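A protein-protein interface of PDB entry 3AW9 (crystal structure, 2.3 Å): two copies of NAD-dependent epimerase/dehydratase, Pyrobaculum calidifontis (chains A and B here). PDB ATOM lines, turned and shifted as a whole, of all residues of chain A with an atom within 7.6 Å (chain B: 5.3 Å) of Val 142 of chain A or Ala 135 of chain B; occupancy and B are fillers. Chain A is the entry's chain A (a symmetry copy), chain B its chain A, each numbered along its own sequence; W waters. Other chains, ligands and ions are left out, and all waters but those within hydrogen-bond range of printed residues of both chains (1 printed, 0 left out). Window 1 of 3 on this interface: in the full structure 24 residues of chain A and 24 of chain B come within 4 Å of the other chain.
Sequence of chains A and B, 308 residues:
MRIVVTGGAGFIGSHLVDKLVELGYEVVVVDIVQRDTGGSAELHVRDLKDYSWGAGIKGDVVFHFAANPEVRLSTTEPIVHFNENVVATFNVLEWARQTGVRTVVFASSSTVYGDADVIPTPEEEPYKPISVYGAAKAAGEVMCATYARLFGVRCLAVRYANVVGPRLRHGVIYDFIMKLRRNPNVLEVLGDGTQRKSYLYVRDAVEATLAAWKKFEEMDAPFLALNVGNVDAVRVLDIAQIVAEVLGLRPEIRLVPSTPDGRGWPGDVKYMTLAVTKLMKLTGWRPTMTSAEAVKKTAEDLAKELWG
The guanidinium group of Arg 149 of chain A is in hydrogen-bond range of the backbone carbonyl oxygen of Pro 129 of chain B (2.9 Å).
The side-chain hydroxyl of Ser 131 of chain B sits at hydrogen-bond distance from the backbone NH of Gly 134 of chain B. OE1 of Glu 141 of chain A is in hydrogen-bond range of OH of Tyr 127 of chain A. OG1 of Thr 146 of chain A is in hydrogen-bond range of O of Val 142 of chain A, at 2.6 Å. SG of Cys 144 of chain A forms a disulfide with SG of Cys 155 of chain A, 2.0 Å away.
Tyr 127 of chain B touches Tyr 127 of chain A. CG1 of Val 142 of chain B touches O of Ala 135 of chain A (3.8 Å). Ala 138 of chain A touches Val 142 of chain B (CB to CG1, 3.8 Å). Val 142 of chain A touches Pro 129 of chain B (CG1 to CG, 3.99 Å). O of Ala 135 of chain B touches CG1 of Val 142 of chain A, at 3.8 Å. CB of Ala 138 of chain B touches CG1 of Val 142 of chain A, at 3.8 Å. Thr 146 of chain A touches Pro 129 of chain B. CG2 of Thr 146 of chain A touches O of Ser 131 of chain B, 3.2 Å away. Thr 146 of chain A touches Ala 135 of chain B (OG1 to CB, 3.5 Å). CG2 of Val 132 of chain B touches CE1 of Tyr 147 of chain A, at 3.98 Å.
Of the printed residues of chain B, Val 142 of chain A touches Pro 129 (3.99 Å), Ala 135 (3.8 Å) and Ala 138 (3.8 Å). No residue of chain A comes within 4 Å of Gly 134 of chain B. Printed residues of chain B within 4 Å of Tyr 127 of chain A: Tyr 127 (3.9 Å). Of the printed residues of chain A, Pro 129 of chain B touches Val 142, Thr 146 and Arg 149. Lys 137 of chain B touches none of the printed residues of chain A. Ala 148 of chain A touches none of the printed residues of chain B. The nearest printed residue of chain B that does not touch Val 142 of chain A is Tyr 127 of chain B (4.3 Å). The nearest residue of chain A that does not touch Ala 135 of chain B is Met 143 of chain A (4.4 Å). The nearest printed residue of chain B that does not touch Arg 149 of chain A is Tyr 127 of chain B (4.4 Å).
Hydrophobic or aromatic side chains of chain B within 4 Å of the printed part of chain A: Tyr 127, Pro 129, Val 132, Ala 135, Ala 138 and Val 142. Along chain B the printed residues that touch a printed residue of chain A span positions 127 to 142. Of the 22 printed residues of chain A, 7 touch a printed residue of chain B. Printed residues of chain A that touch a printed residue of chain B: Tyr 127, Ala 135, Ala 138, Val 142, Thr 146, Tyr 147 and Arg 149. Hydrophobic or aromatic side chains of chain A within 4 Å of the printed part of chain B: Tyr 127, Ala 138, Val 142 and Tyr 147. Along chain A the printed residues that touch a printed residue of chain B span positions 127 to 149. Among the printed residues, no Asp or Glu carboxylate lies within 4 Å of a Lys or Arg side-chain nitrogen of the other chain.
Tyr 127 of chain B touches its own counterpart, Tyr 127 of chain A. Ala 135 of chain A touches Val 142 of chain B, and with the chains exchanged Val 142 of chain A touches Ala 135 of chain B. Ala 138 of chain A touches Val 142 of chain B, and with the chains exchanged Val 142 of chain A touches Ala 138 of chain B. Of the 11 pairs that touch across the chains among the printed residues, 5 have their exchanged pair printed and touching as well.
Water W1 lies within hydrogen-bond range of the guanidinium group (NH2) of Arg 149 of chain A and the backbone carbonyl oxygen (O) of Tyr 127 of chain B.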
ATOM      1  N   LEU A  93     -30.586   0.734 -10.258  1.00  0.00           N
ATOM      2  CA  LEU A  93     -29.392  -0.078 -10.017  1.00  0.00           C
ATOM      3  C   LEU A  93     -28.973  -0.094  -8.557  1.00  0.00           C
ATOM      4  O   LEU A  93     -28.483  -1.102  -8.055  1.00  0.00           O
ATOM      5  CB  LEU A  93     -28.226   0.399 -10.878  1.00  0.00           C
ATOM      6  CG  LEU A  93     -28.342   0.271 -12.403  1.00  0.00           C
ATOM      7  CD1 LEU A  93     -27.274   1.137 -13.033  1.00  0.00           C
ATOM      8  CD2 LEU A  93     -28.230  -1.190 -12.918  1.00  0.00           C
ATOM      9  N   PHE A 106     -32.201  -4.162 -19.146  1.00  0.00           N
ATOM     10  CA  PHE A 106     -32.224  -2.738 -19.400  1.00  0.00           C
ATOM     11  C   PHE A 106     -32.716  -2.414 -20.827  1.00  0.00           C
ATOM     12  O   PHE A 106     -32.086  -2.836 -21.808  1.00  0.00           O
ATOM     13  CB  PHE A 106     -30.813  -2.196 -19.205  1.00  0.00           C
ATOM     14  CG  PHE A 106     -30.677  -0.729 -19.506  1.00  0.00           C
ATOM     15  CD1 PHE A 106     -31.420   0.206 -18.806  1.00  0.00           C
ATOM     16  CD2 PHE A 106     -29.797  -0.289 -20.493  1.00  0.00           C
ATOM     17  CE1 PHE A 106     -31.275   1.571 -19.079  1.00  0.00           C
ATOM     18  CE2 PHE A 106     -29.649   1.066 -20.767  1.00  0.00           C
ATOM     19  CZ  PHE A 106     -30.389   1.997 -20.061  1.00  0.00           C
ATOM     20  N   TYR A 127     -20.146   3.670 -28.832  1.00  0.00           N
ATOM     21  CA  TYR A 127     -21.111   4.711 -28.516  1.00  0.00           C
ATOM     22  C   TYR A 127     -20.737   5.993 -29.252  1.00  0.00           C
ATOM     23  O   TYR A 127     -19.675   6.551 -29.000  1.00  0.00           O
ATOM     24  CB  TYR A 127     -21.131   4.985 -27.017  1.00  0.00           C
ATOM     25  CG  TYR A 127     -21.519   3.812 -26.148  1.00  0.00           C
ATOM     26  CD1 TYR A 127     -22.673   3.079 -26.408  1.00  0.00           C
ATOM     27  CD2 TYR A 127     -20.753   3.460 -25.035  1.00  0.00           C
ATOM     28  CE1 TYR A 127     -23.049   2.023 -25.593  1.00  0.00           C
ATOM     29  CE2 TYR A 127     -21.119   2.381 -24.212  1.00  0.00           C
ATOM     30  CZ  TYR A 127     -22.268   1.674 -24.495  1.00  0.00           C
ATOM     31  OH  TYR A 127     -22.644   0.617 -23.695  1.00  0.00           O
ATOM     32  N   ALA A 135     -27.077   9.459 -25.388  1.00  0.00           N
ATOM     33  CA  ALA A 135     -26.109   9.606 -24.301  1.00  0.00           C
ATOM     34  C   ALA A 135     -26.597   9.028 -22.985  1.00  0.00           C
ATOM     35  O   ALA A 135     -25.836   8.392 -22.280  1.00  0.00           O
ATOM     36  CB  ALA A 135     -25.758  11.078 -24.107  1.00  0.00           C
ATOM     37  N   ALA A 136     -27.857   9.273 -22.653  1.00  0.00           N
ATOM     38  CA  ALA A 136     -28.454   8.776 -21.408  1.00  0.00           C
ATOM     39  C   ALA A 136     -28.599   7.269 -21.450  1.00  0.00           C
ATOM     40  O   ALA A 136     -28.315   6.599 -20.461  1.00  0.00           O
ATOM     41  CB  ALA A 136     -29.806   9.422 -21.170  1.00  0.00           C
ATOM     42  N   LYS A 137     -29.030   6.725 -22.588  1.00  0.00           N
ATOM     43  CA  LYS A 137     -29.039   5.261 -22.726  1.00  0.00           C
ATOM     44  C   LYS A 137     -27.631   4.640 -22.678  1.00  0.00           C
ATOM     45  O   LYS A 137     -27.434   3.625 -22.033  1.00  0.00           O
ATOM     46  CB  LYS A 137     -29.810   4.819 -23.973  1.00  0.00           C
ATOM     47  CG  LYS A 137     -31.318   5.175 -23.928  1.00  0.00           C
ATOM     48  CD  LYS A 137     -32.029   4.420 -22.813  1.00  0.00           C
ATOM     49  CE  LYS A 137     -33.518   4.525 -22.951  1.00  0.00           C
ATOM     50  NZ  LYS A 137     -34.175   3.762 -21.854  1.00  0.00           N
ATOM     51  N   ALA A 138     -26.662   5.260 -23.347  1.00  0.00           N
ATOM     52  CA  ALA A 138     -25.314   4.729 -23.333  1.00  0.00           C
ATOM     53  C   ALA A 138     -24.754   4.794 -21.913  1.00  0.00           C
ATOM     54  O   ALA A 138     -24.076   3.869 -21.492  1.00  0.00           O
ATOM     55  CB  ALA A 138     -24.417   5.480 -24.314  1.00  0.00           C
ATOM     56  N   ALA A 139     -25.059   5.879 -21.188  1.00  0.00           N
ATOM     57  CA  ALA A 139     -24.615   6.069 -19.815  1.00  0.00           C
ATOM     58  C   ALA A 139     -25.219   4.995 -18.900  1.00  0.00           C
ATOM     59  O   ALA A 139     -24.505   4.386 -18.097  1.00  0.00           O
ATOM     60  CB  ALA A 139     -24.992   7.482 -19.317  1.00  0.00           C
ATOM     61  N   GLY A 140     -26.531   4.784 -19.017  1.00  0.00           N
ATOM     62  CA  GLY A 140     -27.241   3.683 -18.376  1.00  0.00           C
ATOM     63  C   GLY A 140     -26.607   2.330 -18.627  1.00  0.00           C
ATOM     64  O   GLY A 140     -26.410   1.557 -17.691  1.00  0.00           O
ATOM     65  N   GLU A 141     -26.290   2.028 -19.885  1.00  0.00           N
ATOM     66  CA  GLU A 141     -25.600   0.772 -20.236  1.00  0.00           C
ATOM     67  C   GLU A 141     -24.272   0.590 -19.511  1.00  0.00           C
ATOM     68  O   GLU A 141     -24.014  -0.459 -18.938  1.00  0.00           O
ATOM     69  CB  GLU A 141     -25.337   0.705 -21.739  1.00  0.00           C
ATOM     70  CG  GLU A 141     -26.518   0.347 -22.586  1.00  0.00           C
ATOM     71  CD  GLU A 141     -26.103  -0.132 -23.991  1.00  0.00           C
ATOM     72  OE1 GLU A 141     -24.913  -0.474 -24.185  1.00  0.00           O
ATOM     73  OE2 GLU A 141     -26.974  -0.181 -24.887  1.00  0.00           O
ATOM     74  N   VAL A 142     -23.430   1.619 -19.552  1.00  0.00           N
ATOM     75  CA  VAL A 142     -22.144   1.618 -18.846  1.00  0.00           C
ATOM     76  C   VAL A 142     -22.316   1.356 -17.334  1.00  0.00           C
ATOM     77  O   VAL A 142     -21.609   0.539 -16.769  1.00  0.00           O
ATOM     78  CB  VAL A 142     -21.366   2.954 -19.120  1.00  0.00           C
ATOM     79  CG1 VAL A 142     -20.158   3.120 -18.182  1.00  0.00           C
ATOM     80  CG2 VAL A 142     -20.918   3.041 -20.623  1.00  0.00           C
ATOM     81  N   MET A 143     -23.266   2.053 -16.696  1.00  0.00           N
ATOM     82  CA  MET A 143     -23.511   1.912 -15.262  1.00  0.00           C
ATOM     83  C   MET A 143     -24.012   0.508 -14.925  1.00  0.00           C
ATOM     84  O   MET A 143     -23.564  -0.068 -13.929  1.00  0.00           O
ATOM     85  CB  MET A 143     -24.515   2.951 -14.722  1.00  0.00           C
ATOM     86  CG  MET A 143     -24.087   4.433 -14.753  1.00  0.00           C
ATOM     87  SD  MET A 143     -25.246   5.633 -13.920  1.00  0.00           S
ATOM     88  CE  MET A 143     -26.725   5.557 -14.955  1.00  0.00           C
ATOM     89  N   CYS A 144     -24.950  -0.029 -15.720  1.00  0.00           N
ATOM     90  CA  CYS A 144     -25.518  -1.361 -15.414  1.00  0.00           C
ATOM     91  C   CYS A 144     -24.499  -2.460 -15.652  1.00  0.00           C
ATOM     92  O   CYS A 144     -24.515  -3.429 -14.946  1.00  0.00           O
ATOM     93  CB  CYS A 144     -26.855  -1.702 -16.144  1.00  0.00           C
ATOM     94  SG  CYS A 144     -26.484  -2.453 -17.681  1.00  0.00           S
ATOM     95  N   ALA A 145     -23.630  -2.286 -16.643  1.00  0.00           N
ATOM     96  CA  ALA A 145     -22.519  -3.203 -16.908  1.00  0.00           C
ATOM     97  C   ALA A 145     -21.519  -3.237 -15.751  1.00  0.00           C
ATOM     98  O   ALA A 145     -21.071  -4.308 -15.317  1.00  0.00           O
ATOM     99  CB  ALA A 145     -21.804  -2.834 -18.222  1.00  0.00           C
ATOM    100  N   THR A 146     -21.194  -2.053 -15.244  1.00  0.00           N
ATOM    101  CA  THR A 146     -20.324  -1.928 -14.104  1.00  0.00           C
ATOM    102  C   THR A 146     -20.893  -2.558 -12.842  1.00  0.00           C
ATOM    103  O   THR A 146     -20.155  -3.233 -12.118  1.00  0.00           O
ATOM    104  CB  THR A 146     -19.959  -0.473 -13.855  1.00  0.00           C
ATOM    105  OG1 THR A 146     -19.619   0.119 -15.101  1.00  0.00           O
ATOM    106  CG2 THR A 146     -18.764  -0.361 -12.886  1.00  0.00           C
ATOM    107  N   TYR A 147     -22.178  -2.331 -12.569  1.00  0.00           N
ATOM    108  CA  TYR A 147     -22.855  -2.989 -11.469  1.00  0.00           C
ATOM    109  C   TYR A 147     -22.813  -4.506 -11.613  1.00  0.00           C
ATOM    110  O   TYR A 147     -22.742  -5.210 -10.609  1.00  0.00           O
ATOM    111  CB  TYR A 147     -24.311  -2.488 -11.319  1.00  0.00           C
ATOM    112  CG  TYR A 147     -24.413  -1.265 -10.433  1.00  0.00           C
ATOM    113  CD1 TYR A 147     -23.762  -0.068 -10.768  1.00  0.00           C
ATOM    114  CD2 TYR A 147     -25.135  -1.305  -9.259  1.00  0.00           C
ATOM    115  CE1 TYR A 147     -23.856   1.065  -9.948  1.00  0.00           C
ATOM    116  CE2 TYR A 147     -25.230  -0.182  -8.422  1.00  0.00           C
ATOM    117  CZ  TYR A 147     -24.587   0.991  -8.773  1.00  0.00           C
ATOM    118  OH  TYR A 147     -24.683   2.056  -7.924  1.00  0.00           O
ATOM    119  N   ALA A 148     -22.874  -4.989 -12.855  1.00  0.00           N
ATOM    120  CA  ALA A 148     -22.711  -6.427 -13.166  1.00  0.00           C
ATOM    121  C   ALA A 148     -21.357  -6.946 -12.752  1.00  0.00           C
ATOM    122  O   ALA A 148     -21.267  -7.969 -12.102  1.00  0.00           O
ATOM    123  CB  ALA A 148     -22.925  -6.713 -14.638  1.00  0.00           C
ATOM    124  N   ARG A 149     -20.313  -6.239 -13.148  1.00  0.00           N
ATOM    125  CA  ARG A 149     -18.953  -6.700 -12.945  1.00  0.00           C
ATOM    126  C   ARG A 149     -18.568  -6.602 -11.467  1.00  0.00           C
ATOM    127  O   ARG A 149     -17.899  -7.482 -10.932  1.00  0.00           O
ATOM    128  CB  ARG A 149     -18.000  -5.895 -13.833  1.00  0.00           C
ATOM    129  CG  ARG A 149     -18.193  -6.171 -15.335  1.00  0.00           C
ATOM    130  CD  ARG A 149     -17.083  -5.568 -16.192  1.00  0.00           C
ATOM    131  NE  ARG A 149     -17.347  -4.171 -16.485  1.00  0.00           N
ATOM    132  CZ  ARG A 149     -17.933  -3.694 -17.589  1.00  0.00           C
ATOM    133  NH1 ARG A 149     -18.324  -4.486 -18.583  1.00  0.00           N
ATOM    134  NH2 ARG A 149     -18.119  -2.391 -17.696  1.00  0.00           N
ATOM    135  N   CYS A 155     -26.418  -7.876 -16.221  1.00  0.00           N
ATOM    136  CA  CYS A 155     -27.134  -6.825 -16.940  1.00  0.00           C
ATOM    137  C   CYS A 155     -27.246  -7.175 -18.408  1.00  0.00           C
ATOM    138  O   CYS A 155     -26.226  -7.302 -19.098  1.00  0.00           O
ATOM    139  CB  CYS A 155     -26.462  -5.451 -16.788  1.00  0.00           C
ATOM    140  SG  CYS A 155     -27.400  -4.248 -17.753  1.00  0.00           S
ATOM    141  N   ALA A 157     -28.456  -5.508 -21.563  1.00  0.00           N
ATOM    142  CA  ALA A 157     -28.823  -4.278 -22.236  1.00  0.00           C
ATOM    143  C   ALA A 157     -29.416  -4.591 -23.609  1.00  0.00           C
ATOM    144  O   ALA A 157     -28.726  -5.082 -24.520  1.00  0.00           O
ATOM    145  CB  ALA A 157     -27.627  -3.342 -22.339  1.00  0.00           C
ATOM    146  N   ARG A 159     -30.762  -3.265 -26.943  1.00  0.00           N
ATOM    147  CA  ARG A 159     -30.792  -2.106 -27.826  1.00  0.00           C
ATOM    148  C   ARG A 159     -31.893  -2.219 -28.879  1.00  0.00           C
ATOM    149  O   ARG A 159     -31.676  -2.778 -29.953  1.00  0.00           O
ATOM    150  CB  ARG A 159     -29.441  -1.890 -28.491  1.00  0.00           C
ATOM    151  CG  ARG A 159     -28.356  -1.563 -27.524  1.00  0.00           C
ATOM    152  CD  ARG A 159     -26.997  -1.860 -28.086  1.00  0.00           C
ATOM    153  NE  ARG A 159     -25.953  -1.530 -27.117  1.00  0.00           N
ATOM    154  CZ  ARG A 159     -24.648  -1.621 -27.362  1.00  0.00           C
ATOM    155  NH1 ARG A 159     -24.227  -2.060 -28.549  1.00  0.00           N
ATOM    156  NH2 ARG A 159     -23.761  -1.304 -26.413  1.00  0.00           N
ATOM    157  N   PHE A 223     -22.244  -8.896 -18.343  1.00  0.00           N
ATOM    158  CA  PHE A 223     -22.938  -7.929 -19.195  1.00  0.00           C
ATOM    159  C   PHE A 223     -23.069  -8.434 -20.626  1.00  0.00           C
ATOM    160  O   PHE A 223     -22.092  -8.932 -21.201  1.00  0.00           O
ATOM    161  CB  PHE A 223     -22.175  -6.596 -19.210  1.00  0.00           C
ATOM    162  CG  PHE A 223     -22.695  -5.599 -20.231  1.00  0.00           C
ATOM    163  CD1 PHE A 223     -23.949  -5.016 -20.079  1.00  0.00           C
ATOM    164  CD2 PHE A 223     -21.912  -5.233 -21.335  1.00  0.00           C
ATOM    165  CE1 PHE A 223     -24.418  -4.090 -21.022  1.00  0.00           C
ATOM    166  CE2 PHE A 223     -22.375  -4.303 -22.280  1.00  0.00           C
ATOM    167  CZ  PHE A 223     -23.621  -3.732 -22.121  1.00  0.00           C
ATOM    168  N   TYR B 127     -15.201   0.913 -23.309  1.00  0.00           N
ATOM    169  CA  TYR B 127     -15.474   1.116 -21.895  1.00  0.00           C
ATOM    170  C   TYR B 127     -15.790  -0.224 -21.240  1.00  0.00           C
ATOM    171  O   TYR B 127     -16.777  -0.857 -21.597  1.00  0.00           O
ATOM    172  CB  TYR B 127     -16.662   2.054 -21.709  1.00  0.00           C
ATOM    173  CG  TYR B 127     -16.486   3.442 -22.279  1.00  0.00           C
ATOM    174  CD1 TYR B 127     -15.360   4.203 -21.981  1.00  0.00           C
ATOM    175  CD2 TYR B 127     -17.473   4.015 -23.086  1.00  0.00           C
ATOM    176  CE1 TYR B 127     -15.214   5.489 -22.476  1.00  0.00           C
ATOM    177  CE2 TYR B 127     -17.325   5.313 -23.604  1.00  0.00           C
ATOM    178  CZ  TYR B 127     -16.197   6.042 -23.290  1.00  0.00           C
ATOM    179  OH  TYR B 127     -16.040   7.318 -23.786  1.00  0.00           O
ATOM    180  N   PRO B 129     -15.412  -0.327 -17.415  1.00  0.00           N
ATOM    181  CA  PRO B 129     -15.010   0.015 -16.033  1.00  0.00           C
ATOM    182  C   PRO B 129     -15.482  -1.011 -14.989  1.00  0.00           C
ATOM    183  O   PRO B 129     -16.521  -1.674 -15.160  1.00  0.00           O
ATOM    184  CB  PRO B 129     -15.704   1.355 -15.789  1.00  0.00           C
ATOM    185  CG  PRO B 129     -16.838   1.404 -16.774  1.00  0.00           C
ATOM    186  CD  PRO B 129     -16.300   0.703 -17.995  1.00  0.00           C
ATOM    187  N   SER B 131     -15.137  -0.095 -11.499  1.00  0.00           N
ATOM    188  CA  SER B 131     -15.561   0.752 -10.394  1.00  0.00           C
ATOM    189  C   SER B 131     -16.668   1.735 -10.823  1.00  0.00           C
ATOM    190  O   SER B 131     -16.799   2.063 -12.013  1.00  0.00           O
ATOM    191  CB  SER B 131     -14.367   1.511  -9.825  1.00  0.00           C
ATOM    192  OG  SER B 131     -13.773   2.351 -10.803  1.00  0.00           O
ATOM    193  N   VAL B 132     -17.466   2.183  -9.851  1.00  0.00           N
ATOM    194  CA  VAL B 132     -18.497   3.190 -10.058  1.00  0.00           C
ATOM    195  C   VAL B 132     -17.890   4.528 -10.508  1.00  0.00           C
ATOM    196  O   VAL B 132     -18.482   5.253 -11.287  1.00  0.00           O
ATOM    197  CB  VAL B 132     -19.437   3.305  -8.791  1.00  0.00           C
ATOM    198  CG1 VAL B 132     -20.421   4.482  -8.894  1.00  0.00           C
ATOM    199  CG2 VAL B 132     -20.230   1.983  -8.602  1.00  0.00           C
ATOM    200  N   TYR B 133     -16.690   4.827 -10.031  1.00  0.00           N
ATOM    201  CA  TYR B 133     -15.876   5.942 -10.495  1.00  0.00           C
ATOM    202  C   TYR B 133     -15.506   5.847 -12.001  1.00  0.00           C
ATOM    203  O   TYR B 133     -15.612   6.837 -12.740  1.00  0.00           O
ATOM    204  CB  TYR B 133     -14.622   6.035  -9.612  1.00  0.00           C
ATOM    205  CG  TYR B 133     -13.591   7.038 -10.070  1.00  0.00           C
ATOM    206  CD1 TYR B 133     -13.733   8.416  -9.801  1.00  0.00           C
ATOM    207  CD2 TYR B 133     -12.470   6.619 -10.781  1.00  0.00           C
ATOM    208  CE1 TYR B 133     -12.745   9.347 -10.224  1.00  0.00           C
ATOM    209  CE2 TYR B 133     -11.500   7.523 -11.197  1.00  0.00           C
ATOM    210  CZ  TYR B 133     -11.638   8.873 -10.924  1.00  0.00           C
ATOM    211  OH  TYR B 133     -10.640   9.715 -11.356  1.00  0.00           O
ATOM    212  N   GLY B 134     -15.069   4.669 -12.451  1.00  0.00           N
ATOM    213  CA  GLY B 134     -14.807   4.449 -13.880  1.00  0.00           C
ATOM    214  C   GLY B 134     -16.020   4.617 -14.781  1.00  0.00           C
ATOM    215  O   GLY B 134     -15.924   5.212 -15.854  1.00  0.00           O
ATOM    216  N   ALA B 135     -17.137   4.032 -14.368  1.00  0.00           N
ATOM    217  CA  ALA B 135     -18.457   4.238 -14.963  1.00  0.00           C
ATOM    218  C   ALA B 135     -18.851   5.702 -15.047  1.00  0.00           C
ATOM    219  O   ALA B 135     -19.402   6.127 -16.045  1.00  0.00           O
ATOM    220  CB  ALA B 135     -19.515   3.476 -14.170  1.00  0.00           C
ATOM    221  N   ALA B 136     -18.586   6.456 -13.990  1.00  0.00           N
ATOM    222  CA  ALA B 136     -18.916   7.885 -13.939  1.00  0.00           C
ATOM    223  C   ALA B 136     -18.050   8.668 -14.903  1.00  0.00           C
ATOM    224  O   ALA B 136     -18.549   9.553 -15.594  1.00  0.00           O
ATOM    225  CB  ALA B 136     -18.743   8.423 -12.531  1.00  0.00           C
ATOM    226  N   LYS B 137     -16.758   8.347 -14.968  1.00  0.00           N
ATOM    227  CA  LYS B 137     -15.914   8.972 -15.997  1.00  0.00           C
ATOM    228  C   LYS B 137     -16.329   8.596 -17.432  1.00  0.00           C
ATOM    229  O   LYS B 137     -16.367   9.451 -18.300  1.00  0.00           O
ATOM    230  CB  LYS B 137     -14.429   8.696 -15.749  1.00  0.00           C
ATOM    231  CG  LYS B 137     -13.894   9.319 -14.434  1.00  0.00           C
ATOM    232  CD  LYS B 137     -13.946  10.840 -14.483  1.00  0.00           C
ATOM    233  CE  LYS B 137     -13.165  11.445 -13.356  1.00  0.00           C
ATOM    234  NZ  LYS B 137     -13.226  12.930 -13.450  1.00  0.00           N
ATOM    235  N   ALA B 138     -16.652   7.326 -17.666  1.00  0.00           N
ATOM    236  CA  ALA B 138     -17.059   6.912 -18.994  1.00  0.00           C
ATOM    237  C   ALA B 138     -18.371   7.603 -19.364  1.00  0.00           C
ATOM    238  O   ALA B 138     -18.534   8.011 -20.504  1.00  0.00           O
ATOM    239  CB  ALA B 138     -17.193   5.394 -19.080  1.00  0.00           C
ATOM    240  N   ALA B 139     -19.282   7.739 -18.390  1.00  0.00           N
ATOM    241  CA  ALA B 139     -20.567   8.394 -18.588  1.00  0.00           C
ATOM    242  C   ALA B 139     -20.368   9.875 -18.937  1.00  0.00           C
ATOM    243  O   ALA B 139     -20.980  10.381 -19.884  1.00  0.00           O
ATOM    244  CB  ALA B 139     -21.449   8.245 -17.329  1.00  0.00           C
ATOM    245  N   GLY B 140     -19.529  10.562 -18.159  1.00  0.00           N
ATOM    246  CA  GLY B 140     -19.072  11.916 -18.448  1.00  0.00           C
ATOM    247  C   GLY B 140     -18.522  12.080 -19.851  1.00  0.00           C
ATOM    248  O   GLY B 140     -18.888  13.022 -20.551  1.00  0.00           O
ATOM    249  N   VAL B 142     -19.081  10.160 -22.582  1.00  0.00           N
ATOM    250  CA  VAL B 142     -20.215  10.009 -23.500  1.00  0.00           C
ATOM    251  C   VAL B 142     -21.064  11.297 -23.586  1.00  0.00           C
ATOM    252  O   VAL B 142     -21.398  11.739 -24.673  1.00  0.00           O
ATOM    253  CB  VAL B 142     -21.085   8.766 -23.098  1.00  0.00           C
ATOM    254  CG1 VAL B 142     -22.429   8.736 -23.846  1.00  0.00           C
ATOM    255  CG2 VAL B 142     -20.291   7.431 -23.331  1.00  0.00           C
HETATM  256  O   HOH W   1     -19.082  -0.885 -19.716  1.00  0.00           O
